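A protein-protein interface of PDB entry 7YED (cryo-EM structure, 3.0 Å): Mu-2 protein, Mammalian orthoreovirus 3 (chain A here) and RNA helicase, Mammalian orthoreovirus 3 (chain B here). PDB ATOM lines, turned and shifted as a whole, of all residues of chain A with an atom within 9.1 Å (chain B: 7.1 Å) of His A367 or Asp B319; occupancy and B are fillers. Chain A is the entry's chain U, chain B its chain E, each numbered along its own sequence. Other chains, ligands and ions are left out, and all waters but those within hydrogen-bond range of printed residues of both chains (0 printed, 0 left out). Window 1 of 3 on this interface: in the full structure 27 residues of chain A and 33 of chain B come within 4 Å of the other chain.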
ATOM      1  N   LEU A 301     -23.585 -29.355  38.381  1.00  0.00           N
ATOM      2  CA  LEU A 301     -22.291 -29.650  37.789  1.00  0.00           C
ATOM      3  C   LEU A 301     -21.516 -30.537  38.753  1.00  0.00           C
ATOM      4  O   LEU A 301     -21.231 -30.127  39.883  1.00  0.00           O
ATOM      5  CB  LEU A 301     -21.515 -28.366  37.502  1.00  0.00           C
ATOM      6  CG  LEU A 301     -22.099 -27.416  36.461  1.00  0.00           C
ATOM      7  CD1 LEU A 301     -21.282 -26.149  36.407  1.00  0.00           C
ATOM      8  CD2 LEU A 301     -22.119 -28.075  35.115  1.00  0.00           C
ATOM      9  N   LYS A 317     -16.461 -35.152  33.690  1.00  0.00           N
ATOM     10  CA  LYS A 317     -17.295 -34.030  34.096  1.00  0.00           C
ATOM     11  C   LYS A 317     -18.648 -34.110  33.402  1.00  0.00           C
ATOM     12  O   LYS A 317     -18.726 -34.447  32.218  1.00  0.00           O
ATOM     13  CB  LYS A 317     -16.614 -32.704  33.771  1.00  0.00           C
ATOM     14  CG  LYS A 317     -15.347 -32.472  34.560  1.00  0.00           C
ATOM     15  CD  LYS A 317     -14.714 -31.142  34.225  1.00  0.00           C
ATOM     16  CE  LYS A 317     -13.503 -30.893  35.099  1.00  0.00           C
ATOM     17  NZ  LYS A 317     -12.417 -31.863  34.810  1.00  0.00           N
ATOM     18  N   LEU A 318     -19.711 -33.791  34.139  1.00  0.00           N
ATOM     19  CA  LEU A 318     -21.067 -34.032  33.666  1.00  0.00           C
ATOM     20  C   LEU A 318     -21.984 -32.896  34.100  1.00  0.00           C
ATOM     21  O   LEU A 318     -21.602 -32.031  34.890  1.00  0.00           O
ATOM     22  CB  LEU A 318     -21.579 -35.378  34.183  1.00  0.00           C
ATOM     23  CG  LEU A 318     -20.778 -36.569  33.663  1.00  0.00           C
ATOM     24  CD1 LEU A 318     -21.204 -37.847  34.341  1.00  0.00           C
ATOM     25  CD2 LEU A 318     -20.941 -36.680  32.164  1.00  0.00           C
ATOM     26  N   ILE A 319     -23.208 -32.907  33.568  1.00  0.00           N
ATOM     27  CA  ILE A 319     -24.218 -31.887  33.845  1.00  0.00           C
ATOM     28  C   ILE A 319     -25.579 -32.568  33.905  1.00  0.00           C
ATOM     29  O   ILE A 319     -25.974 -33.242  32.951  1.00  0.00           O
ATOM     30  CB  ILE A 319     -24.234 -30.786  32.768  1.00  0.00           C
ATOM     31  CG1 ILE A 319     -22.885 -30.087  32.680  1.00  0.00           C
ATOM     32  CG2 ILE A 319     -25.309 -29.767  33.069  1.00  0.00           C
ATOM     33  CD1 ILE A 319     -22.773 -29.175  31.487  1.00  0.00           C
ATOM     34  N   HIS A 321     -28.767 -31.463  33.959  1.00  0.00           N
ATOM     35  CA  HIS A 321     -29.859 -31.064  33.071  1.00  0.00           C
ATOM     36  C   HIS A 321     -31.248 -31.045  33.705  1.00  0.00           C
ATOM     37  O   HIS A 321     -31.990 -32.022  33.596  1.00  0.00           O
ATOM     38  CB  HIS A 321     -29.875 -31.952  31.831  1.00  0.00           C
ATOM     39  CG  HIS A 321     -28.746 -31.676  30.891  1.00  0.00           C
ATOM     40  ND1 HIS A 321     -28.469 -32.474  29.804  1.00  0.00           N
ATOM     41  CD2 HIS A 321     -27.817 -30.694  30.885  1.00  0.00           C
ATOM     42  CE1 HIS A 321     -27.417 -31.993  29.166  1.00  0.00           C
ATOM     43  NE2 HIS A 321     -27.002 -30.912  29.802  1.00  0.00           N
ATOM     44  N   LEU A 361     -27.761 -36.533  31.837  1.00  0.00           N
ATOM     45  CA  LEU A 361     -26.453 -35.944  32.036  1.00  0.00           C
ATOM     46  C   LEU A 361     -25.582 -36.169  30.808  1.00  0.00           C
ATOM     47  O   LEU A 361     -25.496 -37.288  30.299  1.00  0.00           O
ATOM     48  CB  LEU A 361     -25.816 -36.523  33.296  1.00  0.00           C
ATOM     49  CG  LEU A 361     -25.354 -37.970  33.339  1.00  0.00           C
ATOM     50  CD1 LEU A 361     -24.432 -38.199  34.522  1.00  0.00           C
ATOM     51  CD2 LEU A 361     -26.550 -38.865  33.447  1.00  0.00           C
ATOM     52  N   THR A 362     -24.950 -35.098  30.328  1.00  0.00           N
ATOM     53  CA  THR A 362     -24.070 -35.146  29.167  1.00  0.00           C
ATOM     54  C   THR A 362     -22.654 -34.767  29.565  1.00  0.00           C
ATOM     55  O   THR A 362     -22.451 -33.905  30.422  1.00  0.00           O
ATOM     56  CB  THR A 362     -24.543 -34.206  28.050  1.00  0.00           C
ATOM     57  OG1 THR A 362     -24.512 -32.849  28.517  1.00  0.00           O
ATOM     58  CG2 THR A 362     -25.948 -34.563  27.610  1.00  0.00           C
ATOM     59  N   ASP A 363     -21.675 -35.408  28.930  1.00  0.00           N
ATOM     60  CA  ASP A 363     -20.281 -35.096  29.201  1.00  0.00           C
ATOM     61  C   ASP A 363     -19.968 -33.682  28.736  1.00  0.00           C
ATOM     62  O   ASP A 363     -20.455 -33.229  27.697  1.00  0.00           O
ATOM     63  CB  ASP A 363     -19.362 -36.102  28.506  1.00  0.00           C
ATOM     64  CG  ASP A 363     -17.914 -35.989  28.962  1.00  0.00           C
ATOM     65  OD1 ASP A 363     -17.607 -35.095  29.780  1.00  0.00           O
ATOM     66  OD2 ASP A 363     -17.074 -36.797  28.511  1.00  0.00           O
ATOM     67  N   ARG A 364     -19.154 -32.978  29.516  1.00  0.00           N
ATOM     68  CA  ARG A 364     -18.789 -31.612  29.173  1.00  0.00           C
ATOM     69  C   ARG A 364     -17.614 -31.537  28.212  1.00  0.00           C
ATOM     70  O   ARG A 364     -17.456 -30.522  27.528  1.00  0.00           O
ATOM     71  CB  ARG A 364     -18.465 -30.818  30.440  1.00  0.00           C
ATOM     72  CG  ARG A 364     -19.658 -30.615  31.349  1.00  0.00           C
ATOM     73  CD  ARG A 364     -19.278 -29.855  32.602  1.00  0.00           C
ATOM     74  NE  ARG A 364     -18.899 -28.479  32.310  1.00  0.00           N
ATOM     75  CZ  ARG A 364     -18.372 -27.650  33.201  1.00  0.00           C
ATOM     76  NH1 ARG A 364     -18.160 -28.060  34.443  1.00  0.00           N
ATOM     77  NH2 ARG A 364     -18.052 -26.413  32.853  1.00  0.00           N
ATOM     78  N   ARG A 365     -16.789 -32.581  28.146  1.00  0.00           N
ATOM     79  CA  ARG A 365     -15.698 -32.605  27.179  1.00  0.00           C
ATOM     80  C   ARG A 365     -16.237 -32.762  25.764  1.00  0.00           C
ATOM     81  O   ARG A 365     -16.050 -31.888  24.912  1.00  0.00           O
ATOM     82  CB  ARG A 365     -14.724 -33.732  27.524  1.00  0.00           C
ATOM     83  CG  ARG A 365     -13.570 -33.881  26.554  1.00  0.00           C
ATOM     84  CD  ARG A 365     -12.584 -32.734  26.678  1.00  0.00           C
ATOM     85  NE  ARG A 365     -12.966 -31.591  25.859  1.00  0.00           N
ATOM     86  CZ  ARG A 365     -12.363 -30.409  25.904  1.00  0.00           C
ATOM     87  NH1 ARG A 365     -11.348 -30.215  26.732  1.00  0.00           N
ATOM     88  NH2 ARG A 365     -12.777 -29.421  25.123  1.00  0.00           N
ATOM     89  N   THR A 366     -16.914 -33.872  25.496  1.00  0.00           N
ATOM     90  CA  THR A 366     -17.652 -34.061  24.256  1.00  0.00           C
ATOM     91  C   THR A 366     -19.123 -33.822  24.551  1.00  0.00           C
ATOM     92  O   THR A 366     -19.718 -34.536  25.363  1.00  0.00           O
ATOM     93  CB  THR A 366     -17.443 -35.465  23.693  1.00  0.00           C
ATOM     94  OG1 THR A 366     -17.951 -36.430  24.621  1.00  0.00           O
ATOM     95  CG2 THR A 366     -15.970 -35.726  23.470  1.00  0.00           C
ATOM     96  N   HIS A 367     -19.714 -32.832  23.892  1.00  0.00           N
ATOM     97  CA  HIS A 367     -21.072 -32.425  24.228  1.00  0.00           C
ATOM     98  C   HIS A 367     -22.096 -33.442  23.746  1.00  0.00           C
ATOM     99  O   HIS A 367     -22.905 -33.142  22.862  1.00  0.00           O
ATOM    100  CB  HIS A 367     -21.372 -31.054  23.629  1.00  0.00           C
ATOM    101  CG  HIS A 367     -20.520 -29.956  24.179  1.00  0.00           C
ATOM    102  ND1 HIS A 367     -20.729 -29.407  25.424  1.00  0.00           N
ATOM    103  CD2 HIS A 367     -19.456 -29.308  23.654  1.00  0.00           C
ATOM    104  CE1 HIS A 367     -19.831 -28.464  25.642  1.00  0.00           C
ATOM    105  NE2 HIS A 367     -19.045 -28.385  24.584  1.00  0.00           N
ATOM    106  N   CYS A 368     -22.082 -34.640  24.326  1.00  0.00           N
ATOM    107  CA  CYS A 368     -22.997 -35.697  23.933  1.00  0.00           C
ATOM    108  C   CYS A 368     -23.533 -36.382  25.183  1.00  0.00           C
ATOM    109  O   CYS A 368     -22.967 -36.261  26.269  1.00  0.00           O
ATOM    110  CB  CYS A 368     -22.313 -36.710  23.007  1.00  0.00           C
ATOM    111  SG  CYS A 368     -20.942 -37.605  23.756  1.00  0.00           S
ATOM    112  N   GLN A 369     -24.643 -37.097  25.014  1.00  0.00           N
ATOM    113  CA  GLN A 369     -25.286 -37.793  26.121  1.00  0.00           C
ATOM    114  C   GLN A 369     -24.329 -38.794  26.759  1.00  0.00           C
ATOM    115  O   GLN A 369     -23.325 -39.193  26.168  1.00  0.00           O
ATOM    116  CB  GLN A 369     -26.541 -38.506  25.632  1.00  0.00           C
ATOM    117  CG  GLN A 369     -27.627 -37.564  25.185  1.00  0.00           C
ATOM    118  CD  GLN A 369     -28.829 -38.300  24.668  1.00  0.00           C
ATOM    119  OE1 GLN A 369     -28.830 -39.527  24.595  1.00  0.00           O
ATOM    120  NE2 GLN A 369     -29.864 -37.558  24.297  1.00  0.00           N
ATOM    121  N   TYR A 370     -24.639 -39.198  27.992  1.00  0.00           N
ATOM    122  CA  TYR A 370     -23.688 -39.999  28.750  1.00  0.00           C
ATOM    123  C   TYR A 370     -24.186 -41.386  29.134  1.00  0.00           C
ATOM    124  O   TYR A 370     -23.495 -42.372  28.853  1.00  0.00           O
ATOM    125  CB  TYR A 370     -23.242 -39.249  30.000  1.00  0.00           C
ATOM    126  CG  TYR A 370     -22.227 -40.044  30.754  1.00  0.00           C
ATOM    127  CD1 TYR A 370     -20.957 -40.219  30.258  1.00  0.00           C
ATOM    128  CD2 TYR A 370     -22.547 -40.636  31.952  1.00  0.00           C
ATOM    129  CE1 TYR A 370     -20.032 -40.960  30.938  1.00  0.00           C
ATOM    130  CE2 TYR A 370     -21.636 -41.374  32.643  1.00  0.00           C
ATOM    131  CZ  TYR A 370     -20.380 -41.530  32.131  1.00  0.00           C
ATOM    132  OH  TYR A 370     -19.456 -42.271  32.823  1.00  0.00           O
ATOM    133  N   ILE B 232     -17.789 -39.621  18.495  1.00  0.00           N
ATOM    134  CA  ILE B 232     -18.090 -38.348  19.138  1.00  0.00           C
ATOM    135  C   ILE B 232     -18.701 -37.359  18.160  1.00  0.00           C
ATOM    136  O   ILE B 232     -19.754 -36.781  18.427  1.00  0.00           O
ATOM    137  CB  ILE B 232     -16.816 -37.769  19.790  1.00  0.00           C
ATOM    138  CG1 ILE B 232     -16.322 -38.689  20.903  1.00  0.00           C
ATOM    139  CG2 ILE B 232     -17.084 -36.382  20.321  1.00  0.00           C
ATOM    140  CD1 ILE B 232     -14.951 -38.329  21.413  1.00  0.00           C
ATOM    141  N   ARG B 309      -7.866 -18.477  34.350  1.00  0.00           N
ATOM    142  CA  ARG B 309      -8.983 -17.655  34.808  1.00  0.00           C
ATOM    143  C   ARG B 309      -9.419 -18.011  36.225  1.00  0.00           C
ATOM    144  O   ARG B 309     -10.609 -18.011  36.536  1.00  0.00           O
ATOM    145  CB  ARG B 309     -10.172 -17.746  33.854  1.00  0.00           C
ATOM    146  CG  ARG B 309      -9.942 -17.108  32.517  1.00  0.00           C
ATOM    147  CD  ARG B 309     -11.210 -17.132  31.694  1.00  0.00           C
ATOM    148  NE  ARG B 309     -11.587 -18.464  31.244  1.00  0.00           N
ATOM    149  CZ  ARG B 309     -12.700 -19.082  31.615  1.00  0.00           C
ATOM    150  NH1 ARG B 309     -13.545 -18.479  32.438  1.00  0.00           N
ATOM    151  NH2 ARG B 309     -12.971 -20.298  31.162  1.00  0.00           N
ATOM    152  N   PHE B 316     -18.101 -13.009  29.580  1.00  0.00           N
ATOM    153  CA  PHE B 316     -18.559 -14.095  28.726  1.00  0.00           C
ATOM    154  C   PHE B 316     -17.626 -15.280  28.903  1.00  0.00           C
ATOM    155  O   PHE B 316     -16.404 -15.121  28.835  1.00  0.00           O
ATOM    156  CB  PHE B 316     -18.592 -13.661  27.261  1.00  0.00           C
ATOM    157  CG  PHE B 316     -19.068 -14.724  26.325  1.00  0.00           C
ATOM    158  CD1 PHE B 316     -20.407 -15.034  26.238  1.00  0.00           C
ATOM    159  CD2 PHE B 316     -18.178 -15.407  25.519  1.00  0.00           C
ATOM    160  CE1 PHE B 316     -20.849 -16.008  25.372  1.00  0.00           C
ATOM    161  CE2 PHE B 316     -18.616 -16.381  24.653  1.00  0.00           C
ATOM    162  CZ  PHE B 316     -19.951 -16.681  24.580  1.00  0.00           C
ATOM    163  N   ASP B 317     -18.196 -16.455  29.136  1.00  0.00           N
ATOM    164  CA  ASP B 317     -17.409 -17.669  29.289  1.00  0.00           C
ATOM    165  C   ASP B 317     -17.146 -18.287  27.922  1.00  0.00           C
ATOM    166  O   ASP B 317     -18.017 -18.283  27.050  1.00  0.00           O
ATOM    167  CB  ASP B 317     -18.135 -18.667  30.189  1.00  0.00           C
ATOM    168  CG  ASP B 317     -17.268 -19.847  30.574  1.00  0.00           C
ATOM    169  OD1 ASP B 317     -16.104 -19.906  30.130  1.00  0.00           O
ATOM    170  OD2 ASP B 317     -17.751 -20.719  31.324  1.00  0.00           O
ATOM    171  N   ARG B 318     -15.939 -18.815  27.739  1.00  0.00           N
ATOM    172  CA  ARG B 318     -15.553 -19.423  26.474  1.00  0.00           C
ATOM    173  C   ARG B 318     -15.460 -20.940  26.534  1.00  0.00           C
ATOM    174  O   ARG B 318     -15.067 -21.556  25.539  1.00  0.00           O
ATOM    175  CB  ARG B 318     -14.220 -18.848  25.984  1.00  0.00           C
ATOM    176  CG  ARG B 318     -14.293 -17.400  25.549  1.00  0.00           C
ATOM    177  CD  ARG B 318     -12.981 -16.948  24.942  1.00  0.00           C
ATOM    178  NE  ARG B 318     -12.985 -15.524  24.619  1.00  0.00           N
ATOM    179  CZ  ARG B 318     -13.393 -15.016  23.462  1.00  0.00           C
ATOM    180  NH1 ARG B 318     -13.836 -15.812  22.507  1.00  0.00           N
ATOM    181  NH2 ARG B 318     -13.358 -13.710  23.264  1.00  0.00           N
ATOM    182  N   ASP B 319     -15.759 -21.551  27.681  1.00  0.00           N
ATOM    183  CA  ASP B 319     -15.914 -22.999  27.820  1.00  0.00           C
ATOM    184  C   ASP B 319     -14.579 -23.735  27.762  1.00  0.00           C
ATOM    185  O   ASP B 319     -14.509 -24.931  28.058  1.00  0.00           O
ATOM    186  CB  ASP B 319     -16.855 -23.535  26.738  1.00  0.00           C
ATOM    187  CG  ASP B 319     -17.362 -24.927  27.043  1.00  0.00           C
ATOM    188  OD1 ASP B 319     -17.037 -25.460  28.121  1.00  0.00           O
ATOM    189  OD2 ASP B 319     -18.086 -25.496  26.200  1.00  0.00           O
ATOM    190  N   SER B 320     -13.511 -23.030  27.419  1.00  0.00           N
ATOM    191  CA  SER B 320     -12.182 -23.608  27.425  1.00  0.00           C
ATOM    192  C   SER B 320     -11.543 -23.334  28.772  1.00  0.00           C
ATOM    193  O   SER B 320     -11.741 -22.268  29.357  1.00  0.00           O
ATOM    194  CB  SER B 320     -11.332 -23.023  26.302  1.00  0.00           C
ATOM    195  OG  SER B 320     -11.881 -23.346  25.039  1.00  0.00           O
ATOM    196  N   SER B 321     -10.809 -24.313  29.283  1.00  0.00           N
ATOM    197  CA  SER B 321     -10.125 -24.125  30.553  1.00  0.00           C
ATOM    198  C   SER B 321      -9.095 -25.216  30.772  1.00  0.00           C
ATOM    199  O   SER B 321      -9.427 -26.403  30.754  1.00  0.00           O
ATOM    200  CB  SER B 321     -11.122 -24.111  31.712  1.00  0.00           C
ATOM    201  OG  SER B 321     -11.964 -22.975  31.667  1.00  0.00           O
ATOM    202  N   GLU B 364      -6.434 -24.965  23.646  1.00  0.00           N
ATOM    203  CA  GLU B 364      -7.397 -24.568  24.672  1.00  0.00           C
ATOM    204  C   GLU B 364      -6.860 -23.432  25.523  1.00  0.00           C
ATOM    205  O   GLU B 364      -7.590 -22.492  25.859  1.00  0.00           O
ATOM    206  CB  GLU B 364      -7.747 -25.746  25.576  1.00  0.00           C
ATOM    207  CG  GLU B 364      -8.629 -26.808  24.976  1.00  0.00           C
ATOM    208  CD  GLU B 364      -8.911 -27.916  25.967  1.00  0.00           C
ATOM    209  OE1 GLU B 364      -8.291 -27.911  27.051  1.00  0.00           O
ATOM    210  OE2 GLU B 364      -9.754 -28.783  25.666  1.00  0.00           O
ATOM    211  N   LEU B 367      -7.129 -20.222  23.512  1.00  0.00           N
ATOM    212  CA  LEU B 367      -8.511 -19.800  23.311  1.00  0.00           C
ATOM    213  C   LEU B 367      -9.174 -19.348  24.601  1.00  0.00           C
ATOM    214  O   LEU B 367     -10.148 -18.595  24.551  1.00  0.00           O
ATOM    215  CB  LEU B 367      -9.334 -20.930  22.697  1.00  0.00           C
ATOM    216  CG  LEU B 367      -9.036 -21.367  21.267  1.00  0.00           C
ATOM    217  CD1 LEU B 367      -9.864 -22.582  20.920  1.00  0.00           C
ATOM    218  CD2 LEU B 367      -9.325 -20.243  20.306  1.00  0.00           C
ATOM    219  N   ASP B 368      -8.686 -19.802  25.755  1.00  0.00           N
ATOM    220  CA  ASP B 368      -9.378 -19.488  26.998  1.00  0.00           C
ATOM    221  C   ASP B 368      -9.280 -18.012  27.331  1.00  0.00           C
ATOM    222  O   ASP B 368     -10.267 -17.402  27.755  1.00  0.00           O
ATOM    223  CB  ASP B 368      -8.822 -20.326  28.140  1.00  0.00           C
ATOM    224  CG  ASP B 368      -9.675 -20.242  29.385  1.00  0.00           C
ATOM    225  OD1 ASP B 368     -10.685 -19.508  29.380  1.00  0.00           O
ATOM    226  OD2 ASP B 368      -9.354 -20.938  30.368  1.00  0.00           O
ATOM    227  N   TYR B 371      -9.421 -12.197  25.648  1.00  0.00           N
ATOM    228  CA  TYR B 371     -10.277 -11.288  26.387  1.00  0.00           C
ATOM    229  C   TYR B 371      -9.772  -9.878  26.209  1.00  0.00           C
ATOM    230  O   TYR B 371      -8.928  -9.609  25.351  1.00  0.00           O
ATOM    231  CB  TYR B 371     -10.310 -11.619  27.870  1.00  0.00           C
ATOM    232  CG  TYR B 371     -11.061 -12.863  28.228  1.00  0.00           C
ATOM    233  CD1 TYR B 371     -11.974 -13.436  27.362  1.00  0.00           C
ATOM    234  CD2 TYR B 371     -10.846 -13.468  29.439  1.00  0.00           C
ATOM    235  CE1 TYR B 371     -12.648 -14.580  27.705  1.00  0.00           C
ATOM    236  CE2 TYR B 371     -11.507 -14.590  29.783  1.00  0.00           C
ATOM    237  CZ  TYR B 371     -12.405 -15.152  28.924  1.00  0.00           C
ATOM    238  OH  TYR B 371     -13.050 -16.297  29.317  1.00  0.00           O
ATOM    239  N   THR B 971     -14.039 -28.387  16.699  1.00  0.00           N
ATOM    240  CA  THR B 971     -15.022 -28.313  17.769  1.00  0.00           C
ATOM    241  C   THR B 971     -14.605 -27.309  18.832  1.00  0.00           C
ATOM    242  O   THR B 971     -15.441 -26.562  19.348  1.00  0.00           O
ATOM    243  CB  THR B 971     -15.236 -29.688  18.389  1.00  0.00           C
ATOM    244  OG1 THR B 971     -15.745 -30.581  17.393  1.00  0.00           O
ATOM    245  CG2 THR B 971     -16.221 -29.599  19.528  1.00  0.00           C
ATOM    246  N   THR B 975     -16.709 -23.988  19.834  1.00  0.00           N
ATOM    247  CA  THR B 975     -17.129 -23.775  21.214  1.00  0.00           C
ATOM    248  C   THR B 975     -16.728 -22.388  21.689  1.00  0.00           C
ATOM    249  O   THR B 975     -17.559 -21.628  22.195  1.00  0.00           O
ATOM    250  CB  THR B 975     -16.531 -24.847  22.118  1.00  0.00           C
ATOM    251  OG1 THR B 975     -16.995 -26.135  21.701  1.00  0.00           O
ATOM    252  CG2 THR B 975     -16.936 -24.609  23.556  1.00  0.00           C
ATOM    253  N   ALA B 976     -15.456 -22.038  21.536  1.00  0.00           N
ATOM    254  CA  ALA B 976     -15.107 -20.636  21.661  1.00  0.00           C
ATOM    255  C   ALA B 976     -15.734 -19.862  20.508  1.00  0.00           C
ATOM    256  O   ALA B 976     -16.107 -20.429  19.482  1.00  0.00           O
ATOM    257  CB  ALA B 976     -13.593 -20.447  21.677  1.00  0.00           C
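OD1 of Asp B317 sits at hydrogen-bond distance from N of Asp B319 (3.0 Å). OD1 of Asp A363 lies within hydrogen-bond range of N of Arg A365, 3.1 Å away. The side-chain sulfur (SG) of Cys A368 lies within hydrogen-bond range of the side-chain hydroxyl (OG1) of Thr A366 (3.3 Å).
Thr A366 touches Ile B232 (CG2 to CG2, 3.4 Å).
Printed residues of chain B within 4 Å of Thr A366: Ile B232 (3.4 Å). His A367 touches just one residue of chain B: Asp B319. Printed residues of chain A within 4 Å of Ile B232: Thr A366. No residue of chain A comes within 4 Å of Ser B320. Of the printed residues of chain A, Glu B364 touches Arg A365 (2.4 Å). The nearest residue of chain B that does not touch His A367 is Thr B975 (4.2 Å). The nearest residue of chain A that does not touch Asp B319 is Arg A364 (4.9 Å).
The side-chain carboxylate of Asp B319 is in hydrogen-bond range of a ring nitrogen (NE2) of His A367, at 3.4 Å. The side-chain carboxylate of Glu B364 lies within salt-bridge range of the guanidinium group of Arg A365, 3.1 Å away.
Of the 15 printed residues of chain A, 3 touch a printed residue of chain B. Hydrophobic or aromatic side chains of chain A within 4 Å of the printed part of chain B: His A367. Hydrophobic or aromatic side chains of chain B within 4 Å of the printed part of chain A: Ile B232. Along chain B the printed residues that touch a printed residue of chain A span positions 232 to 364. Among the printed residues, Asp or Glu carboxylates within 4 Å of a Lys or Arg side-chain nitrogen of the other chain: Arg A365 with Glu B364 (2.4 Å).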
